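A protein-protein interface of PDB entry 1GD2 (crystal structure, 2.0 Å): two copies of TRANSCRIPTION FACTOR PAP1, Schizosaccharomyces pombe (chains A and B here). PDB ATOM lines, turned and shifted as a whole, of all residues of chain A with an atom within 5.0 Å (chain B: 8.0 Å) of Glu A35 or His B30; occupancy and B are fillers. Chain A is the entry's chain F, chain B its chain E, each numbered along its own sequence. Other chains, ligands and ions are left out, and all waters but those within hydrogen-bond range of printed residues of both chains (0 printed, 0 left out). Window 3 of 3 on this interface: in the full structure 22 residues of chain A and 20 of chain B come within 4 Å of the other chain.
A ring nitrogen (NE2) of His B30 is in hydrogen-bond range of the side-chain carboxylate of Glu A35.
Among the printed residues, pairs that only touch across the chains: Gln A37 with Val B38 (3.2 Å), Glu A35 with Leu B34 (3.3 Å), Val A38 with Val B38 (3.3 Å), Leu A34 with Glu B35 (3.4 Å), Leu A31 with Leu B34 (3.6 Å), Val A38 with Gln B37 (3.7 Å), Val A38 with Leu B34 (3.8 Å), Leu A34 with Val B38 (3.9 Å) and Leu A34 with Leu B31 (3.9 Å).
Of the printed residues of chain B, Leu A31 touches Leu B34. Ala A33 touches none of the printed residues of chain B. Of the printed residues of chain B, Leu A34 touches Leu B31, Glu B35 and Val B38. Of chain B, only His B30 (2.8 Å) and Leu B34 (3.3 Å) come within 4 Å of Glu A35. Phe B23 touches none of the printed residues of chain A. Of the printed residues of chain A, Leu B31 touches Leu A34. Of the printed residues of chain A, Glu B35 touches Leu A34.
Of the 16 printed residues of chain B, 6 touch a printed residue of chain A. Printed residues of chain B that touch a printed residue of chain A: His B30, Leu B31, Leu B34, Glu B35, Gln B37 and Val B38. Hydrophobic or aromatic side chains of chain B that line the printed part of chain A: His B30, Leu B31, Leu B34 and Val B38. Of the 9 printed residues of chain A, 5 touch a printed residue of chain B. Printed residues of chain A that touch a printed residue of chain B: Leu A31, Leu A34, Glu A35, Gln A37 and Val A38. Among the printed residues, 10 pairs touch across the chains. Among the printed residues, no Asp or Glu carboxylate lies within 4 Å of a Lys or Arg side-chain nitrogen of the other chain.
Leu A31 touches Leu B34, and with the chains exchanged Leu A34 touches Leu B31. Leu A34 touches Glu B35, and with the chains exchanged Glu A35 touches Leu B34. Leu A34 touches Val B38, and with the chains exchanged Val A38 touches Leu B34. Val A38 touches its own counterpart, Val B38.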
ATOM      1  N   LEU A  31     -32.524 -18.448   5.910  1.00  0.00           N
ATOM      2  CA  LEU A  31     -31.199 -18.589   6.498  1.00  0.00           C
ATOM      3  C   LEU A  31     -30.174 -17.876   5.634  1.00  0.00           C
ATOM      4  O   LEU A  31     -29.328 -17.140   6.137  1.00  0.00           O
ATOM      5  CB  LEU A  31     -30.826 -20.068   6.632  1.00  0.00           C
ATOM      6  CG  LEU A  31     -29.426 -20.416   7.156  1.00  0.00           C
ATOM      7  CD1 LEU A  31     -29.209 -19.815   8.546  1.00  0.00           C
ATOM      8  CD2 LEU A  31     -29.252 -21.937   7.194  1.00  0.00           C
ATOM      9  N   LYS A  32     -30.260 -18.111   4.328  1.00  0.00           N
ATOM     10  CA  LYS A  32     -29.356 -17.493   3.368  1.00  0.00           C
ATOM     11  C   LYS A  32     -29.579 -15.981   3.310  1.00  0.00           C
ATOM     12  O   LYS A  32     -28.629 -15.225   3.121  1.00  0.00           O
ATOM     13  CB  LYS A  32     -29.535 -18.138   1.988  1.00  0.00           C
ATOM     14  CG  LYS A  32     -29.126 -19.616   1.961  1.00  0.00           C
ATOM     15  CD  LYS A  32     -29.504 -20.316   0.650  1.00  0.00           C
ATOM     16  CE  LYS A  32     -29.209 -21.818   0.737  1.00  0.00           C
ATOM     17  NZ  LYS A  32     -29.829 -22.623  -0.359  1.00  0.00           N
ATOM     18  N   ALA A  33     -30.828 -15.555   3.508  1.00  0.00           N
ATOM     19  CA  ALA A  33     -31.189 -14.139   3.506  1.00  0.00           C
ATOM     20  C   ALA A  33     -30.631 -13.431   4.742  1.00  0.00           C
ATOM     21  O   ALA A  33     -30.315 -12.248   4.680  1.00  0.00           O
ATOM     22  CB  ALA A  33     -32.696 -13.971   3.435  1.00  0.00           C
ATOM     23  N   LEU A  34     -30.536 -14.148   5.864  1.00  0.00           N
ATOM     24  CA  LEU A  34     -29.988 -13.589   7.101  1.00  0.00           C
ATOM     25  C   LEU A  34     -28.466 -13.511   7.021  1.00  0.00           C
ATOM     26  O   LEU A  34     -27.857 -12.580   7.555  1.00  0.00           O
ATOM     27  CB  LEU A  34     -30.357 -14.446   8.313  1.00  0.00           C
ATOM     28  CG  LEU A  34     -31.769 -14.462   8.895  1.00  0.00           C
ATOM     29  CD1 LEU A  34     -31.808 -15.531   9.988  1.00  0.00           C
ATOM     30  CD2 LEU A  34     -32.161 -13.093   9.457  1.00  0.00           C
ATOM     31  N   GLU A  35     -27.853 -14.516   6.395  1.00  0.00           N
ATOM     32  CA  GLU A  35     -26.400 -14.566   6.242  1.00  0.00           C
ATOM     33  C   GLU A  35     -25.914 -13.393   5.400  1.00  0.00           C
ATOM     34  O   GLU A  35     -24.842 -12.834   5.647  1.00  0.00           O
ATOM     35  CB  GLU A  35     -25.965 -15.877   5.579  1.00  0.00           C
ATOM     36  CG  GLU A  35     -26.256 -17.135   6.386  1.00  0.00           C
ATOM     37  CD  GLU A  35     -25.382 -17.301   7.624  1.00  0.00           C
ATOM     38  OE1 GLU A  35     -24.667 -16.354   8.022  1.00  0.00           O
ATOM     39  OE2 GLU A  35     -25.417 -18.403   8.210  1.00  0.00           O
ATOM     40  N   THR A  36     -26.706 -13.045   4.392  1.00  0.00           N
ATOM     41  CA  THR A  36     -26.385 -11.938   3.508  1.00  0.00           C
ATOM     42  C   THR A  36     -26.667 -10.610   4.213  1.00  0.00           C
ATOM     43  O   THR A  36     -25.936  -9.643   4.016  1.00  0.00           O
ATOM     44  CB  THR A  36     -27.180 -12.039   2.194  1.00  0.00           C
ATOM     45  OG1 THR A  36     -26.963 -13.330   1.613  1.00  0.00           O
ATOM     46  CG2 THR A  36     -26.717 -10.985   1.203  1.00  0.00           C
ATOM     47  N   GLN A  37     -27.708 -10.572   5.049  1.00  0.00           N
ATOM     48  CA  GLN A  37     -28.056  -9.362   5.791  1.00  0.00           C
ATOM     49  C   GLN A  37     -26.948  -8.978   6.763  1.00  0.00           C
ATOM     50  O   GLN A  37     -26.621  -7.799   6.878  1.00  0.00           O
ATOM     51  CB  GLN A  37     -29.379  -9.514   6.558  1.00  0.00           C
ATOM     52  CG  GLN A  37     -30.633  -9.312   5.720  1.00  0.00           C
ATOM     53  CD  GLN A  37     -31.923  -9.357   6.536  1.00  0.00           C
ATOM     54  OE1 GLN A  37     -31.925  -9.724   7.711  1.00  0.00           O
ATOM     55  NE2 GLN A  37     -33.027  -8.988   5.905  1.00  0.00           N
ATOM     56  N   VAL A  38     -26.366  -9.956   7.459  1.00  0.00           N
ATOM     57  CA  VAL A  38     -25.288  -9.649   8.401  1.00  0.00           C
ATOM     58  C   VAL A  38     -24.059  -9.103   7.678  1.00  0.00           C
ATOM     59  O   VAL A  38     -23.432  -8.158   8.149  1.00  0.00           O
ATOM     60  CB  VAL A  38     -24.882 -10.855   9.298  1.00  0.00           C
ATOM     61  CG1 VAL A  38     -26.039 -11.283  10.162  1.00  0.00           C
ATOM     62  CG2 VAL A  38     -24.381 -12.011   8.466  1.00  0.00           C
ATOM     63  N   VAL A  39     -23.734  -9.686   6.527  1.00  0.00           N
ATOM     64  CA  VAL A  39     -22.593  -9.237   5.746  1.00  0.00           C
ATOM     65  C   VAL A  39     -22.868  -7.836   5.198  1.00  0.00           C
ATOM     66  O   VAL A  39     -22.006  -6.967   5.254  1.00  0.00           O
ATOM     67  CB  VAL A  39     -22.276 -10.214   4.599  1.00  0.00           C
ATOM     68  CG1 VAL A  39     -21.098  -9.702   3.783  1.00  0.00           C
ATOM     69  CG2 VAL A  39     -21.954 -11.589   5.166  1.00  0.00           C
ATOM     70  N   PHE B  23     -27.373 -32.460  15.263  1.00  0.00           N
ATOM     71  CA  PHE B  23     -27.228 -31.647  14.056  1.00  0.00           C
ATOM     72  C   PHE B  23     -28.295 -30.556  14.054  1.00  0.00           C
ATOM     73  O   PHE B  23     -27.998 -29.400  13.752  1.00  0.00           O
ATOM     74  CB  PHE B  23     -27.371 -32.530  12.809  1.00  0.00           C
ATOM     75  CG  PHE B  23     -27.222 -31.786  11.505  1.00  0.00           C
ATOM     76  CD1 PHE B  23     -25.980 -31.686  10.885  1.00  0.00           C
ATOM     77  CD2 PHE B  23     -28.329 -31.204  10.886  1.00  0.00           C
ATOM     78  CE1 PHE B  23     -25.843 -31.015   9.665  1.00  0.00           C
ATOM     79  CE2 PHE B  23     -28.201 -30.534   9.671  1.00  0.00           C
ATOM     80  CZ  PHE B  23     -26.957 -30.439   9.060  1.00  0.00           C
ATOM     81  N   ARG B  24     -29.530 -30.937  14.382  1.00  0.00           N
ATOM     82  CA  ARG B  24     -30.656 -30.006  14.450  1.00  0.00           C
ATOM     83  C   ARG B  24     -30.394 -28.912  15.493  1.00  0.00           C
ATOM     84  O   ARG B  24     -30.666 -27.736  15.256  1.00  0.00           O
ATOM     85  CB  ARG B  24     -31.938 -30.755  14.820  1.00  0.00           C
ATOM     86  CG  ARG B  24     -32.879 -31.024  13.667  1.00  0.00           C
ATOM     87  CD  ARG B  24     -34.131 -31.725  14.169  1.00  0.00           C
ATOM     88  NE  ARG B  24     -34.145 -33.142  13.808  1.00  0.00           N
ATOM     89  CZ  ARG B  24     -34.230 -34.148  14.672  1.00  0.00           C
ATOM     90  NH1 ARG B  24     -34.315 -33.919  15.975  1.00  0.00           N
ATOM     91  NH2 ARG B  24     -34.212 -35.392  14.228  1.00  0.00           N
ATOM     92  N   LYS B  25     -29.879 -29.317  16.651  1.00  0.00           N
ATOM     93  CA  LYS B  25     -29.565 -28.399  17.739  1.00  0.00           C
ATOM     94  C   LYS B  25     -28.549 -27.335  17.284  1.00  0.00           C
ATOM     95  O   LYS B  25     -28.774 -26.147  17.476  1.00  0.00           O
ATOM     96  CB  LYS B  25     -29.042 -29.199  18.940  1.00  0.00           C
ATOM     97  CG  LYS B  25     -28.652 -28.389  20.173  1.00  0.00           C
ATOM     98  CD  LYS B  25     -29.810 -27.577  20.729  1.00  0.00           C
ATOM     99  CE  LYS B  25     -29.494 -27.066  22.141  1.00  0.00           C
ATOM    100  NZ  LYS B  25     -28.218 -26.287  22.217  1.00  0.00           N
ATOM    101  N   ARG B  26     -27.457 -27.768  16.658  1.00  0.00           N
ATOM    102  CA  ARG B  26     -26.426 -26.865  16.162  1.00  0.00           C
ATOM    103  C   ARG B  26     -26.981 -25.897  15.121  1.00  0.00           C
ATOM    104  O   ARG B  26     -26.618 -24.722  15.103  1.00  0.00           O
ATOM    105  CB  ARG B  26     -25.257 -27.644  15.546  1.00  0.00           C
ATOM    106  CG  ARG B  26     -24.409 -28.412  16.553  1.00  0.00           C
ATOM    107  CD  ARG B  26     -23.118 -28.939  15.929  1.00  0.00           C
ATOM    108  NE  ARG B  26     -23.322 -29.956  14.888  1.00  0.00           N
ATOM    109  CZ  ARG B  26     -23.499 -31.260  15.115  1.00  0.00           C
ATOM    110  NH1 ARG B  26     -23.509 -31.737  16.352  1.00  0.00           N
ATOM    111  NH2 ARG B  26     -23.619 -32.104  14.097  1.00  0.00           N
ATOM    112  N   LYS B  27     -27.857 -26.399  14.256  1.00  0.00           N
ATOM    113  CA  LYS B  27     -28.471 -25.600  13.203  1.00  0.00           C
ATOM    114  C   LYS B  27     -29.395 -24.521  13.796  1.00  0.00           C
ATOM    115  O   LYS B  27     -29.417 -23.382  13.332  1.00  0.00           O
ATOM    116  CB  LYS B  27     -29.248 -26.533  12.265  1.00  0.00           C
ATOM    117  CG  LYS B  27     -29.557 -25.990  10.882  1.00  0.00           C
ATOM    118  CD  LYS B  27     -30.057 -27.116   9.981  1.00  0.00           C
ATOM    119  CE  LYS B  27     -30.180 -26.699   8.519  1.00  0.00           C
ATOM    120  NZ  LYS B  27     -30.401 -27.888   7.631  1.00  0.00           N
ATOM    121  N   GLU B  28     -30.134 -24.885  14.840  1.00  0.00           N
ATOM    122  CA  GLU B  28     -31.050 -23.962  15.504  1.00  0.00           C
ATOM    123  C   GLU B  28     -30.299 -22.940  16.366  1.00  0.00           C
ATOM    124  O   GLU B  28     -30.727 -21.790  16.479  1.00  0.00           O
ATOM    125  CB  GLU B  28     -32.075 -24.737  16.340  1.00  0.00           C
ATOM    126  CG  GLU B  28     -33.160 -23.879  17.012  1.00  0.00           C
ATOM    127  CD  GLU B  28     -33.922 -22.966  16.038  1.00  0.00           C
ATOM    128  OE1 GLU B  28     -34.523 -23.481  15.059  1.00  0.00           O
ATOM    129  OE2 GLU B  28     -33.924 -21.727  16.265  1.00  0.00           O
ATOM    130  N   ASP B  29     -29.192 -23.354  16.981  1.00  0.00           N
ATOM    131  CA  ASP B  29     -28.391 -22.443  17.794  1.00  0.00           C
ATOM    132  C   ASP B  29     -27.827 -21.346  16.893  1.00  0.00           C
ATOM    133  O   ASP B  29     -27.753 -20.183  17.286  1.00  0.00           O
ATOM    134  CB  ASP B  29     -27.250 -23.189  18.497  1.00  0.00           C
ATOM    135  CG  ASP B  29     -27.731 -24.054  19.652  1.00  0.00           C
ATOM    136  OD1 ASP B  29     -26.966 -24.943  20.074  1.00  0.00           O
ATOM    137  OD2 ASP B  29     -28.863 -23.850  20.144  1.00  0.00           O
ATOM    138  N   HIS B  30     -27.456 -21.720  15.673  1.00  0.00           N
ATOM    139  CA  HIS B  30     -26.923 -20.766  14.718  1.00  0.00           C
ATOM    140  C   HIS B  30     -28.030 -19.847  14.208  1.00  0.00           C
ATOM    141  O   HIS B  30     -27.781 -18.680  13.913  1.00  0.00           O
ATOM    142  CB  HIS B  30     -26.261 -21.488  13.544  1.00  0.00           C
ATOM    143  CG  HIS B  30     -25.643 -20.563  12.541  1.00  0.00           C
ATOM    144  ND1 HIS B  30     -24.827 -19.512  12.900  1.00  0.00           N
ATOM    145  CD2 HIS B  30     -25.723 -20.530  11.189  1.00  0.00           C
ATOM    146  CE1 HIS B  30     -24.431 -18.872  11.815  1.00  0.00           C
ATOM    147  NE2 HIS B  30     -24.960 -19.470  10.763  1.00  0.00           N
ATOM    148  N   LEU B  31     -29.246 -20.373  14.102  1.00  0.00           N
ATOM    149  CA  LEU B  31     -30.378 -19.587  13.631  1.00  0.00           C
ATOM    150  C   LEU B  31     -30.686 -18.473  14.631  1.00  0.00           C
ATOM    151  O   LEU B  31     -30.741 -17.310  14.251  1.00  0.00           O
ATOM    152  CB  LEU B  31     -31.598 -20.490  13.394  1.00  0.00           C
ATOM    153  CG  LEU B  31     -32.840 -20.014  12.618  1.00  0.00           C
ATOM    154  CD1 LEU B  31     -33.830 -19.318  13.536  1.00  0.00           C
ATOM    155  CD2 LEU B  31     -32.439 -19.125  11.448  1.00  0.00           C
ATOM    156  N   LYS B  32     -30.820 -18.824  15.909  1.00  0.00           N
ATOM    157  CA  LYS B  32     -31.108 -17.852  16.970  1.00  0.00           C
ATOM    158  C   LYS B  32     -30.036 -16.768  17.095  1.00  0.00           C
ATOM    159  O   LYS B  32     -30.351 -15.612  17.383  1.00  0.00           O
ATOM    160  CB  LYS B  32     -31.272 -18.557  18.322  1.00  0.00           C
ATOM    161  CG  LYS B  32     -32.484 -19.465  18.400  1.00  0.00           C
ATOM    162  CD  LYS B  32     -32.585 -20.154  19.752  1.00  0.00           C
ATOM    163  CE  LYS B  32     -33.788 -21.094  19.791  1.00  0.00           C
ATOM    164  NZ  LYS B  32     -33.875 -21.865  21.067  1.00  0.00           N
ATOM    165  N   ALA B  33     -28.776 -17.162  16.899  1.00  0.00           N
ATOM    166  CA  ALA B  33     -27.621 -16.262  16.967  1.00  0.00           C
ATOM    167  C   ALA B  33     -27.665 -15.231  15.833  1.00  0.00           C
ATOM    168  O   ALA B  33     -27.428 -14.041  16.058  1.00  0.00           O
ATOM    169  CB  ALA B  33     -26.328 -17.066  16.896  1.00  0.00           C
ATOM    170  N   LEU B  34     -27.957 -15.705  14.622  1.00  0.00           N
ATOM    171  CA  LEU B  34     -28.060 -14.852  13.445  1.00  0.00           C
ATOM    172  C   LEU B  34     -29.220 -13.887  13.599  1.00  0.00           C
ATOM    173  O   LEU B  34     -29.109 -12.712  13.265  1.00  0.00           O
ATOM    174  CB  LEU B  34     -28.295 -15.690  12.189  1.00  0.00           C
ATOM    175  CG  LEU B  34     -27.116 -16.174  11.356  1.00  0.00           C
ATOM    176  CD1 LEU B  34     -27.674 -16.963  10.191  1.00  0.00           C
ATOM    177  CD2 LEU B  34     -26.293 -15.002  10.857  1.00  0.00           C
ATOM    178  N   GLU B  35     -30.348 -14.405  14.068  1.00  0.00           N
ATOM    179  CA  GLU B  35     -31.536 -13.592  14.269  1.00  0.00           C
ATOM    180  C   GLU B  35     -31.239 -12.468  15.246  1.00  0.00           C
ATOM    181  O   GLU B  35     -31.679 -11.339  15.051  1.00  0.00           O
ATOM    182  CB  GLU B  35     -32.683 -14.450  14.798  1.00  0.00           C
ATOM    183  CG  GLU B  35     -33.173 -15.511  13.828  1.00  0.00           C
ATOM    184  CD  GLU B  35     -34.017 -14.960  12.689  1.00  0.00           C
ATOM    185  OE1 GLU B  35     -34.126 -13.725  12.528  1.00  0.00           O
ATOM    186  OE2 GLU B  35     -34.586 -15.782  11.945  1.00  0.00           O
ATOM    187  N   THR B  36     -30.482 -12.790  16.290  1.00  0.00           N
ATOM    188  CA  THR B  36     -30.103 -11.820  17.307  1.00  0.00           C
ATOM    189  C   THR B  36     -29.131 -10.805  16.721  1.00  0.00           C
ATOM    190  O   THR B  36     -29.303  -9.600  16.895  1.00  0.00           O
ATOM    191  CB  THR B  36     -29.446 -12.515  18.512  1.00  0.00           C
ATOM    192  OG1 THR B  36     -30.395 -13.395  19.120  1.00  0.00           O
ATOM    193  CG2 THR B  36     -28.976 -11.495  19.540  1.00  0.00           C
ATOM    194  N   GLN B  37     -28.129 -11.299  16.002  1.00  0.00           N
ATOM    195  CA  GLN B  37     -27.132 -10.440  15.391  1.00  0.00           C
ATOM    196  C   GLN B  37     -27.723  -9.501  14.351  1.00  0.00           C
ATOM    197  O   GLN B  37     -27.306  -8.354  14.263  1.00  0.00           O
ATOM    198  CB  GLN B  37     -26.011 -11.263  14.766  1.00  0.00           C
ATOM    199  CG  GLN B  37     -24.902 -10.396  14.198  1.00  0.00           C
ATOM    200  CD  GLN B  37     -23.812 -11.181  13.498  1.00  0.00           C
ATOM    201  OE1 GLN B  37     -22.716 -10.663  13.276  1.00  0.00           O
ATOM    202  NE2 GLN B  37     -24.105 -12.427  13.135  1.00  0.00           N
ATOM    203  N   VAL B  38     -28.677  -9.982  13.558  1.00  0.00           N
ATOM    204  CA  VAL B  38     -29.308  -9.143  12.539  1.00  0.00           C
ATOM    205  C   VAL B  38     -30.135  -8.029  13.183  1.00  0.00           C
ATOM    206  O   VAL B  38     -30.285  -6.951  12.607  1.00  0.00           O
ATOM    207  CB  VAL B  38     -30.182  -9.970  11.566  1.00  0.00           C
ATOM    208  CG1 VAL B  38     -31.028  -9.060  10.690  1.00  0.00           C
ATOM    209  CG2 VAL B  38     -29.299 -10.822  10.690  1.00  0.00           C
